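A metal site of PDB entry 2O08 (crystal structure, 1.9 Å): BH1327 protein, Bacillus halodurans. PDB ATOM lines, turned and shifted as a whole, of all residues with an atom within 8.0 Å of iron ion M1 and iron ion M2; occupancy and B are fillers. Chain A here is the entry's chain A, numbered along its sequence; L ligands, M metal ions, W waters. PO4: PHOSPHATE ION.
Arg 134 touches iron ion M2 (NH2 to FE, 3.96 Å). Within 4 Å of iron ion M2: His 22, His 51, Asp 52, Asp 128 and Arg 134.
Water W1 is bound to iron ion M1 (2.1 Å). O2 of the ligand binds iron ion M1 (2.1 Å). OD1 of Asp 52 is bound to iron ion M1, at 2.1 Å. A ring nitrogen (NE2) of His 84 is bound to iron ion M1 (2.2 Å). A ring nitrogen (NE2) of His 110 is bound to iron ion M1 (2.2 Å). Iron ion M1 is bound by water W2, at 2.3 Å.
Water W1 binds iron ion M2 (1.8 Å). Iron ion M2 is bound by O3 of the ligand. Iron ion M2 is bound by NE2 of His 22, at 2.2 Å. Iron ion M2 is bound by the side-chain carboxylate (OD2) of Asp 52. Iron ion M2 is bound by OD1 of Asp 128 (2.2 Å). Iron ion M2 is bound by NE2 of His 51 (2.2 Å).
Thr 111 touches iron ion M1. Along chain A the residues within 4 Å of iron ion M1 span positions 52 to 111. The nearest printed residue that does not touch iron ion M1 is His 51 (4.1 Å).
The guanidinium group of Arg 134 is in salt-bridge range of the side-chain carboxylate of Asp 128. The side-chain hydroxyl (OG1) of Thr 111 sits close to a ring nitrogen (NE2) of His 110, at 3.3 Å. O of Ala 48 is in hydrogen-bond range of ND1 of His 51 (2.7 Å). The backbone carbonyl oxygen (O) of Ile 107 lies within hydrogen-bond range of a ring nitrogen (ND1) of His 110 (2.7 Å). The guanidinium group of Arg 19 sits close to the side-chain carboxylate of Asp 52. The side-chain carboxylate (OE2) of Glu 131 lies within hydrogen-bond range of a ring nitrogen (ND1) of His 22. The backbone carbonyl oxygen of Glu 81 sits at hydrogen-bond distance from a ring nitrogen (ND1) of His 84 (3.0 Å).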
ATOM      1  N   ARG A  19     -17.292 -11.176 -32.253  1.00  0.00           N
ATOM      2  CA  ARG A  19     -16.570  -9.947 -32.572  1.00  0.00           C
ATOM      3  C   ARG A  19     -17.528  -8.786 -32.866  1.00  0.00           C
ATOM      4  O   ARG A  19     -17.227  -7.628 -32.542  1.00  0.00           O
ATOM      5  CB  ARG A  19     -15.582 -10.163 -33.732  1.00  0.00           C
ATOM      6  CG  ARG A  19     -14.452 -11.163 -33.383  1.00  0.00           C
ATOM      7  CD  ARG A  19     -13.648 -10.847 -32.118  1.00  0.00           C
ATOM      8  NE  ARG A  19     -12.935  -9.581 -32.196  1.00  0.00           N
ATOM      9  CZ  ARG A  19     -12.067  -9.133 -31.276  1.00  0.00           C
ATOM     10  NH1 ARG A  19     -11.722  -9.849 -30.202  1.00  0.00           N
ATOM     11  NH2 ARG A  19     -11.478  -7.966 -31.457  1.00  0.00           N
ATOM     12  N   HIS A  22     -18.511  -7.528 -29.535  1.00  0.00           N
ATOM     13  CA  HIS A  22     -17.395  -6.728 -29.023  1.00  0.00           C
ATOM     14  C   HIS A  22     -17.423  -5.299 -29.570  1.00  0.00           C
ATOM     15  O   HIS A  22     -17.254  -4.329 -28.818  1.00  0.00           O
ATOM     16  CB  HIS A  22     -16.050  -7.394 -29.379  1.00  0.00           C
ATOM     17  CG  HIS A  22     -14.849  -6.590 -28.987  1.00  0.00           C
ATOM     18  ND1 HIS A  22     -14.583  -6.256 -27.677  1.00  0.00           N
ATOM     19  CD2 HIS A  22     -13.837  -6.085 -29.726  1.00  0.00           C
ATOM     20  CE1 HIS A  22     -13.442  -5.574 -27.624  1.00  0.00           C
ATOM     21  NE2 HIS A  22     -12.981  -5.449 -28.851  1.00  0.00           N
ATOM     22  N   THR A  23     -17.663  -5.161 -30.878  1.00  0.00           N
ATOM     23  CA  THR A  23     -17.626  -3.864 -31.556  1.00  0.00           C
ATOM     24  C   THR A  23     -18.686  -2.933 -31.027  1.00  0.00           C
ATOM     25  O   THR A  23     -18.404  -1.770 -30.667  1.00  0.00           O
ATOM     26  CB  THR A  23     -17.797  -4.064 -33.102  1.00  0.00           C
ATOM     27  OG1 THR A  23     -16.803  -5.005 -33.547  1.00  0.00           O
ATOM     28  CG2 THR A  23     -17.660  -2.722 -33.913  1.00  0.00           C
ATOM     29  N   VAL A  26     -17.859  -1.982 -27.412  1.00  0.00           N
ATOM     30  CA  VAL A  26     -16.818  -0.897 -27.363  1.00  0.00           C
ATOM     31  C   VAL A  26     -17.419   0.466 -27.784  1.00  0.00           C
ATOM     32  O   VAL A  26     -17.179   1.528 -27.139  1.00  0.00           O
ATOM     33  CB  VAL A  26     -15.578  -1.256 -28.201  1.00  0.00           C
ATOM     34  CG1 VAL A  26     -14.525  -0.117 -28.173  1.00  0.00           C
ATOM     35  CG2 VAL A  26     -14.983  -2.536 -27.690  1.00  0.00           C
ATOM     36  N   ALA A  48     -14.217   3.698 -32.088  1.00  0.00           N
ATOM     37  CA  ALA A  48     -14.669   2.408 -31.528  1.00  0.00           C
ATOM     38  C   ALA A  48     -15.066   1.390 -32.571  1.00  0.00           C
ATOM     39  O   ALA A  48     -14.600   0.254 -32.522  1.00  0.00           O
ATOM     40  CB  ALA A  48     -15.775   2.603 -30.559  1.00  0.00           C
ATOM     41  N   HIS A  51     -11.731   0.374 -34.236  1.00  0.00           N
ATOM     42  CA  HIS A  51     -10.490   0.149 -33.463  1.00  0.00           C
ATOM     43  C   HIS A  51      -9.756  -1.184 -33.798  1.00  0.00           C
ATOM     44  O   HIS A  51      -8.518  -1.226 -33.828  1.00  0.00           O
ATOM     45  CB  HIS A  51     -10.706   0.294 -31.949  1.00  0.00           C
ATOM     46  CG  HIS A  51     -11.282  -0.906 -31.294  1.00  0.00           C
ATOM     47  ND1 HIS A  51     -12.612  -1.251 -31.420  1.00  0.00           N
ATOM     48  CD2 HIS A  51     -10.717  -1.843 -30.487  1.00  0.00           C
ATOM     49  CE1 HIS A  51     -12.836  -2.373 -30.745  1.00  0.00           C
ATOM     50  NE2 HIS A  51     -11.713  -2.736 -30.151  1.00  0.00           N
ATOM     51  N   ASP A  52     -10.519  -2.215 -34.089  1.00  0.00           N
ATOM     52  CA  ASP A  52      -9.978  -3.549 -34.386  1.00  0.00           C
ATOM     53  C   ASP A  52     -10.064  -3.937 -35.849  1.00  0.00           C
ATOM     54  O   ASP A  52      -9.989  -5.130 -36.189  1.00  0.00           O
ATOM     55  CB  ASP A  52     -10.660  -4.636 -33.547  1.00  0.00           C
ATOM     56  CG  ASP A  52     -10.080  -4.738 -32.132  1.00  0.00           C
ATOM     57  OD1 ASP A  52      -8.941  -4.382 -31.903  1.00  0.00           O
ATOM     58  OD2 ASP A  52     -10.789  -5.193 -31.243  1.00  0.00           O
ATOM     59  N   TYR A  53     -10.128  -2.925 -36.711  1.00  0.00           N
ATOM     60  CA  TYR A  53     -10.163  -3.137 -38.147  1.00  0.00           C
ATOM     61  C   TYR A  53      -9.136  -4.142 -38.680  1.00  0.00           C
ATOM     62  O   TYR A  53      -9.453  -4.925 -39.581  1.00  0.00           O
ATOM     63  CB  TYR A  53      -9.961  -1.803 -38.844  1.00  0.00           C
ATOM     64  CG  TYR A  53     -10.000  -1.843 -40.328  1.00  0.00           C
ATOM     65  CD1 TYR A  53     -11.217  -1.934 -41.016  1.00  0.00           C
ATOM     66  CD2 TYR A  53      -8.819  -1.733 -41.074  1.00  0.00           C
ATOM     67  CE1 TYR A  53     -11.249  -1.908 -42.434  1.00  0.00           C
ATOM     68  CE2 TYR A  53      -8.848  -1.691 -42.455  1.00  0.00           C
ATOM     69  CZ  TYR A  53     -10.057  -1.754 -43.131  1.00  0.00           C
ATOM     70  OH  TYR A  53     -10.001  -1.749 -44.507  1.00  0.00           O
ATOM     71  N   ALA A  54      -7.902  -4.076 -38.188  1.00  0.00           N
ATOM     72  CA  ALA A  54      -6.810  -4.937 -38.684  1.00  0.00           C
ATOM     73  C   ALA A  54      -6.582  -6.223 -37.848  1.00  0.00           C
ATOM     74  O   ALA A  54      -5.637  -6.949 -38.080  1.00  0.00           O
ATOM     75  CB  ALA A  54      -5.516  -4.111 -38.779  1.00  0.00           C
ATOM     76  N   LYS A  55      -7.457  -6.515 -36.884  1.00  0.00           N
ATOM     77  CA  LYS A  55      -7.235  -7.657 -35.978  1.00  0.00           C
ATOM     78  C   LYS A  55      -6.941  -8.941 -36.754  1.00  0.00           C
ATOM     79  O   LYS A  55      -6.048  -9.683 -36.397  1.00  0.00           O
ATOM     80  CB  LYS A  55      -8.464  -7.809 -35.082  1.00  0.00           C
ATOM     81  CG  LYS A  55      -8.472  -8.947 -34.118  1.00  0.00           C
ATOM     82  CD  LYS A  55      -7.750  -8.677 -32.855  1.00  0.00           C
ATOM     83  CE  LYS A  55      -7.898  -9.900 -31.956  1.00  0.00           C
ATOM     84  NZ  LYS A  55      -7.224  -9.555 -30.706  1.00  0.00           N
ATOM     85  N   GLU A  81       0.046  -9.423 -30.794  1.00  0.00           N
ATOM     86  CA  GLU A  81      -1.137  -8.655 -30.413  1.00  0.00           C
ATOM     87  C   GLU A  81      -0.950  -7.148 -30.593  1.00  0.00           C
ATOM     88  O   GLU A  81      -1.933  -6.430 -30.692  1.00  0.00           O
ATOM     89  CB  GLU A  81      -1.575  -8.978 -28.962  1.00  0.00           C
ATOM     90  N   HIS A  84      -2.018  -5.018 -34.634  1.00  0.00           N
ATOM     91  CA  HIS A  84      -3.246  -4.579 -35.263  1.00  0.00           C
ATOM     92  C   HIS A  84      -3.651  -3.144 -34.990  1.00  0.00           C
ATOM     93  O   HIS A  84      -4.318  -2.550 -35.826  1.00  0.00           O
ATOM     94  CB  HIS A  84      -4.407  -5.549 -34.949  1.00  0.00           C
ATOM     95  CG  HIS A  84      -4.919  -5.475 -33.546  1.00  0.00           C
ATOM     96  ND1 HIS A  84      -4.338  -6.169 -32.505  1.00  0.00           N
ATOM     97  CD2 HIS A  84      -6.003  -4.863 -33.040  1.00  0.00           C
ATOM     98  CE1 HIS A  84      -5.018  -5.933 -31.398  1.00  0.00           C
ATOM     99  NE2 HIS A  84      -6.046  -5.148 -31.696  1.00  0.00           N
ATOM    100  N   ALA A  85      -3.252  -2.583 -33.846  1.00  0.00           N
ATOM    101  CA  ALA A  85      -3.597  -1.175 -33.540  1.00  0.00           C
ATOM    102  C   ALA A  85      -2.913  -0.175 -34.498  1.00  0.00           C
ATOM    103  O   ALA A  85      -3.596   0.609 -35.151  1.00  0.00           O
ATOM    104  CB  ALA A  85      -3.307  -0.816 -32.026  1.00  0.00           C
ATOM    105  N   ILE A 107      -7.207   4.784 -32.395  1.00  0.00           N
ATOM    106  CA  ILE A 107      -7.098   3.432 -32.885  1.00  0.00           C
ATOM    107  C   ILE A 107      -5.678   2.919 -32.625  1.00  0.00           C
ATOM    108  O   ILE A 107      -5.502   1.820 -32.129  1.00  0.00           O
ATOM    109  CB  ILE A 107      -7.450   3.340 -34.392  1.00  0.00           C
ATOM    110  CG1 ILE A 107      -8.922   3.668 -34.621  1.00  0.00           C
ATOM    111  CG2 ILE A 107      -7.131   1.932 -34.913  1.00  0.00           C
ATOM    112  CD1 ILE A 107      -9.326   3.831 -36.095  1.00  0.00           C
ATOM    113  N   HIS A 110      -4.707   1.919 -28.802  1.00  0.00           N
ATOM    114  CA  HIS A 110      -5.741   1.307 -27.964  1.00  0.00           C
ATOM    115  C   HIS A 110      -5.289   0.047 -27.283  1.00  0.00           C
ATOM    116  O   HIS A 110      -5.944  -0.391 -26.326  1.00  0.00           O
ATOM    117  CB  HIS A 110      -7.048   1.002 -28.741  1.00  0.00           C
ATOM    118  CG  HIS A 110      -7.017  -0.257 -29.549  1.00  0.00           C
ATOM    119  ND1 HIS A 110      -6.669  -0.282 -30.893  1.00  0.00           N
ATOM    120  CD2 HIS A 110      -7.316  -1.528 -29.218  1.00  0.00           C
ATOM    121  CE1 HIS A 110      -6.764  -1.539 -31.332  1.00  0.00           C
ATOM    122  NE2 HIS A 110      -7.149  -2.309 -30.327  1.00  0.00           N
ATOM    123  N   THR A 111      -4.273  -0.609 -27.861  1.00  0.00           N
ATOM    124  CA  THR A 111      -3.747  -1.860 -27.283  1.00  0.00           C
ATOM    125  C   THR A 111      -2.639  -1.590 -26.231  1.00  0.00           C
ATOM    126  O   THR A 111      -2.682  -2.157 -25.161  1.00  0.00           O
ATOM    127  CB  THR A 111      -3.126  -2.777 -28.336  1.00  0.00           C
ATOM    128  OG1 THR A 111      -4.085  -3.045 -29.341  1.00  0.00           O
ATOM    129  CG2 THR A 111      -2.649  -4.091 -27.697  1.00  0.00           C
ATOM    130  N   THR A 112      -1.641  -0.778 -26.579  1.00  0.00           N
ATOM    131  CA  THR A 112      -0.500  -0.579 -25.707  1.00  0.00           C
ATOM    132  C   THR A 112      -0.647   0.619 -24.760  1.00  0.00           C
ATOM    133  O   THR A 112      -0.070   0.615 -23.668  1.00  0.00           O
ATOM    134  CB  THR A 112       0.751  -0.352 -26.499  1.00  0.00           C
ATOM    135  OG1 THR A 112       0.637   0.869 -27.255  1.00  0.00           O
ATOM    136  CG2 THR A 112       1.081  -1.589 -27.410  1.00  0.00           C
ATOM    137  N   ILE A 124     -11.060   5.155 -25.806  1.00  0.00           N
ATOM    138  CA  ILE A 124     -11.014   3.938 -26.643  1.00  0.00           C
ATOM    139  C   ILE A 124     -10.222   2.825 -25.975  1.00  0.00           C
ATOM    140  O   ILE A 124     -10.660   1.667 -25.954  1.00  0.00           O
ATOM    141  CB  ILE A 124     -10.531   4.224 -28.097  1.00  0.00           C
ATOM    142  CG1 ILE A 124     -11.473   5.216 -28.786  1.00  0.00           C
ATOM    143  CG2 ILE A 124     -10.440   2.902 -28.941  1.00  0.00           C
ATOM    144  CD1 ILE A 124     -12.981   4.778 -28.857  1.00  0.00           C
ATOM    145  N   PHE A 125      -9.066   3.153 -25.407  1.00  0.00           N
ATOM    146  CA  PHE A 125      -8.289   2.208 -24.645  1.00  0.00           C
ATOM    147  C   PHE A 125      -9.147   1.543 -23.581  1.00  0.00           C
ATOM    148  O   PHE A 125      -9.215   0.312 -23.446  1.00  0.00           O
ATOM    149  CB  PHE A 125      -7.086   2.930 -23.950  1.00  0.00           C
ATOM    150  CG  PHE A 125      -6.220   1.999 -23.155  1.00  0.00           C
ATOM    151  CD1 PHE A 125      -6.566   1.635 -21.844  1.00  0.00           C
ATOM    152  CD2 PHE A 125      -5.078   1.423 -23.732  1.00  0.00           C
ATOM    153  CE1 PHE A 125      -5.777   0.703 -21.144  1.00  0.00           C
ATOM    154  CE2 PHE A 125      -4.299   0.531 -23.028  1.00  0.00           C
ATOM    155  CZ  PHE A 125      -4.646   0.171 -21.744  1.00  0.00           C
ATOM    156  N   ALA A 127     -12.509   1.681 -23.109  1.00  0.00           N
ATOM    157  CA  ALA A 127     -13.776   1.108 -23.636  1.00  0.00           C
ATOM    158  C   ALA A 127     -13.549  -0.325 -24.106  1.00  0.00           C
ATOM    159  O   ALA A 127     -14.344  -1.198 -23.876  1.00  0.00           O
ATOM    160  CB  ALA A 127     -14.317   1.998 -24.749  1.00  0.00           C
ATOM    161  N   ASP A 128     -12.389  -0.574 -24.694  1.00  0.00           N
ATOM    162  CA  ASP A 128     -11.998  -1.901 -25.167  1.00  0.00           C
ATOM    163  C   ASP A 128     -11.885  -2.879 -24.027  1.00  0.00           C
ATOM    164  O   ASP A 128     -12.255  -4.021 -24.130  1.00  0.00           O
ATOM    165  CB  ASP A 128     -10.637  -1.824 -25.827  1.00  0.00           C
ATOM    166  CG  ASP A 128     -10.258  -3.120 -26.538  1.00  0.00           C
ATOM    167  OD1 ASP A 128     -11.118  -3.755 -27.169  1.00  0.00           O
ATOM    168  OD2 ASP A 128      -9.117  -3.566 -26.447  1.00  0.00           O
ATOM    169  N   TYR A 129     -11.379  -2.373 -22.909  1.00  0.00           N
ATOM    170  CA  TYR A 129     -11.121  -3.180 -21.756  1.00  0.00           C
ATOM    171  C   TYR A 129     -12.360  -3.488 -20.939  1.00  0.00           C
ATOM    172  O   TYR A 129     -12.500  -4.616 -20.463  1.00  0.00           O
ATOM    173  CB  TYR A 129     -10.084  -2.433 -20.912  1.00  0.00           C
ATOM    174  CG  TYR A 129      -9.484  -3.298 -19.880  1.00  0.00           C
ATOM    175  CD1 TYR A 129      -8.392  -4.121 -20.171  1.00  0.00           C
ATOM    176  CD2 TYR A 129     -10.012  -3.298 -18.616  1.00  0.00           C
ATOM    177  CE1 TYR A 129      -7.842  -4.924 -19.203  1.00  0.00           C
ATOM    178  CE2 TYR A 129      -9.473  -4.047 -17.662  1.00  0.00           C
ATOM    179  CZ  TYR A 129      -8.404  -4.882 -17.941  1.00  0.00           C
ATOM    180  OH  TYR A 129      -7.931  -5.639 -16.919  1.00  0.00           O
ATOM    181  N   GLU A 131     -15.753  -3.037 -21.953  1.00  0.00           N
ATOM    182  CA  GLU A 131     -17.034  -3.228 -22.663  1.00  0.00           C
ATOM    183  C   GLU A 131     -17.751  -4.445 -22.057  1.00  0.00           C
ATOM    184  O   GLU A 131     -17.082  -5.369 -21.574  1.00  0.00           O
ATOM    185  CB  GLU A 131     -16.839  -3.337 -24.179  1.00  0.00           C
ATOM    186  CG  GLU A 131     -16.092  -4.562 -24.664  1.00  0.00           C
ATOM    187  CD  GLU A 131     -16.952  -5.743 -25.056  1.00  0.00           C
ATOM    188  OE1 GLU A 131     -18.177  -5.741 -24.810  1.00  0.00           O
ATOM    189  OE2 GLU A 131     -16.369  -6.699 -25.636  1.00  0.00           O
ATOM    190  N   ARG A 134     -16.652  -8.290 -21.900  1.00  0.00           N
ATOM    191  CA  ARG A 134     -15.357  -8.673 -21.354  1.00  0.00           C
ATOM    192  C   ARG A 134     -15.528  -9.253 -19.953  1.00  0.00           C
ATOM    193  O   ARG A 134     -16.258  -8.700 -19.147  1.00  0.00           O
ATOM    194  CB  ARG A 134     -14.433  -7.479 -21.279  1.00  0.00           C
ATOM    195  CG  ARG A 134     -14.050  -6.904 -22.590  1.00  0.00           C
ATOM    196  CD  ARG A 134     -13.154  -7.827 -23.400  1.00  0.00           C
ATOM    197  NE  ARG A 134     -12.155  -7.002 -24.066  1.00  0.00           N
ATOM    198  CZ  ARG A 134     -11.589  -7.232 -25.247  1.00  0.00           C
ATOM    199  NH1 ARG A 134     -11.919  -8.273 -26.006  1.00  0.00           N
ATOM    200  NH2 ARG A 134     -10.692  -6.363 -25.675  1.00  0.00           N
HETATM  201  P   PO4 L   1      -8.980  -7.226 -28.818  1.00  0.00           P
HETATM  202  O1  PO4 L   1      -9.210  -8.664 -29.165  1.00  0.00           O
HETATM  203  O2  PO4 L   1      -8.099  -6.522 -29.847  1.00  0.00           O
HETATM  204  O3  PO4 L   1     -10.334  -6.524 -28.743  1.00  0.00           O
HETATM  205  O4  PO4 L   1      -8.344  -7.341 -27.446  1.00  0.00           O
HETATM  206 FE    FE M   1      -7.608  -4.504 -30.249  1.00  0.00          FE
HETATM  207 FE    FE M   2     -11.044  -4.566 -29.185  1.00  0.00          FE
HETATM  208  O   HOH W   1      -9.241  -4.322 -28.997  1.00  0.00           O
HETATM  209  O   HOH W   2      -6.024  -4.524 -28.589  1.00  0.00           O
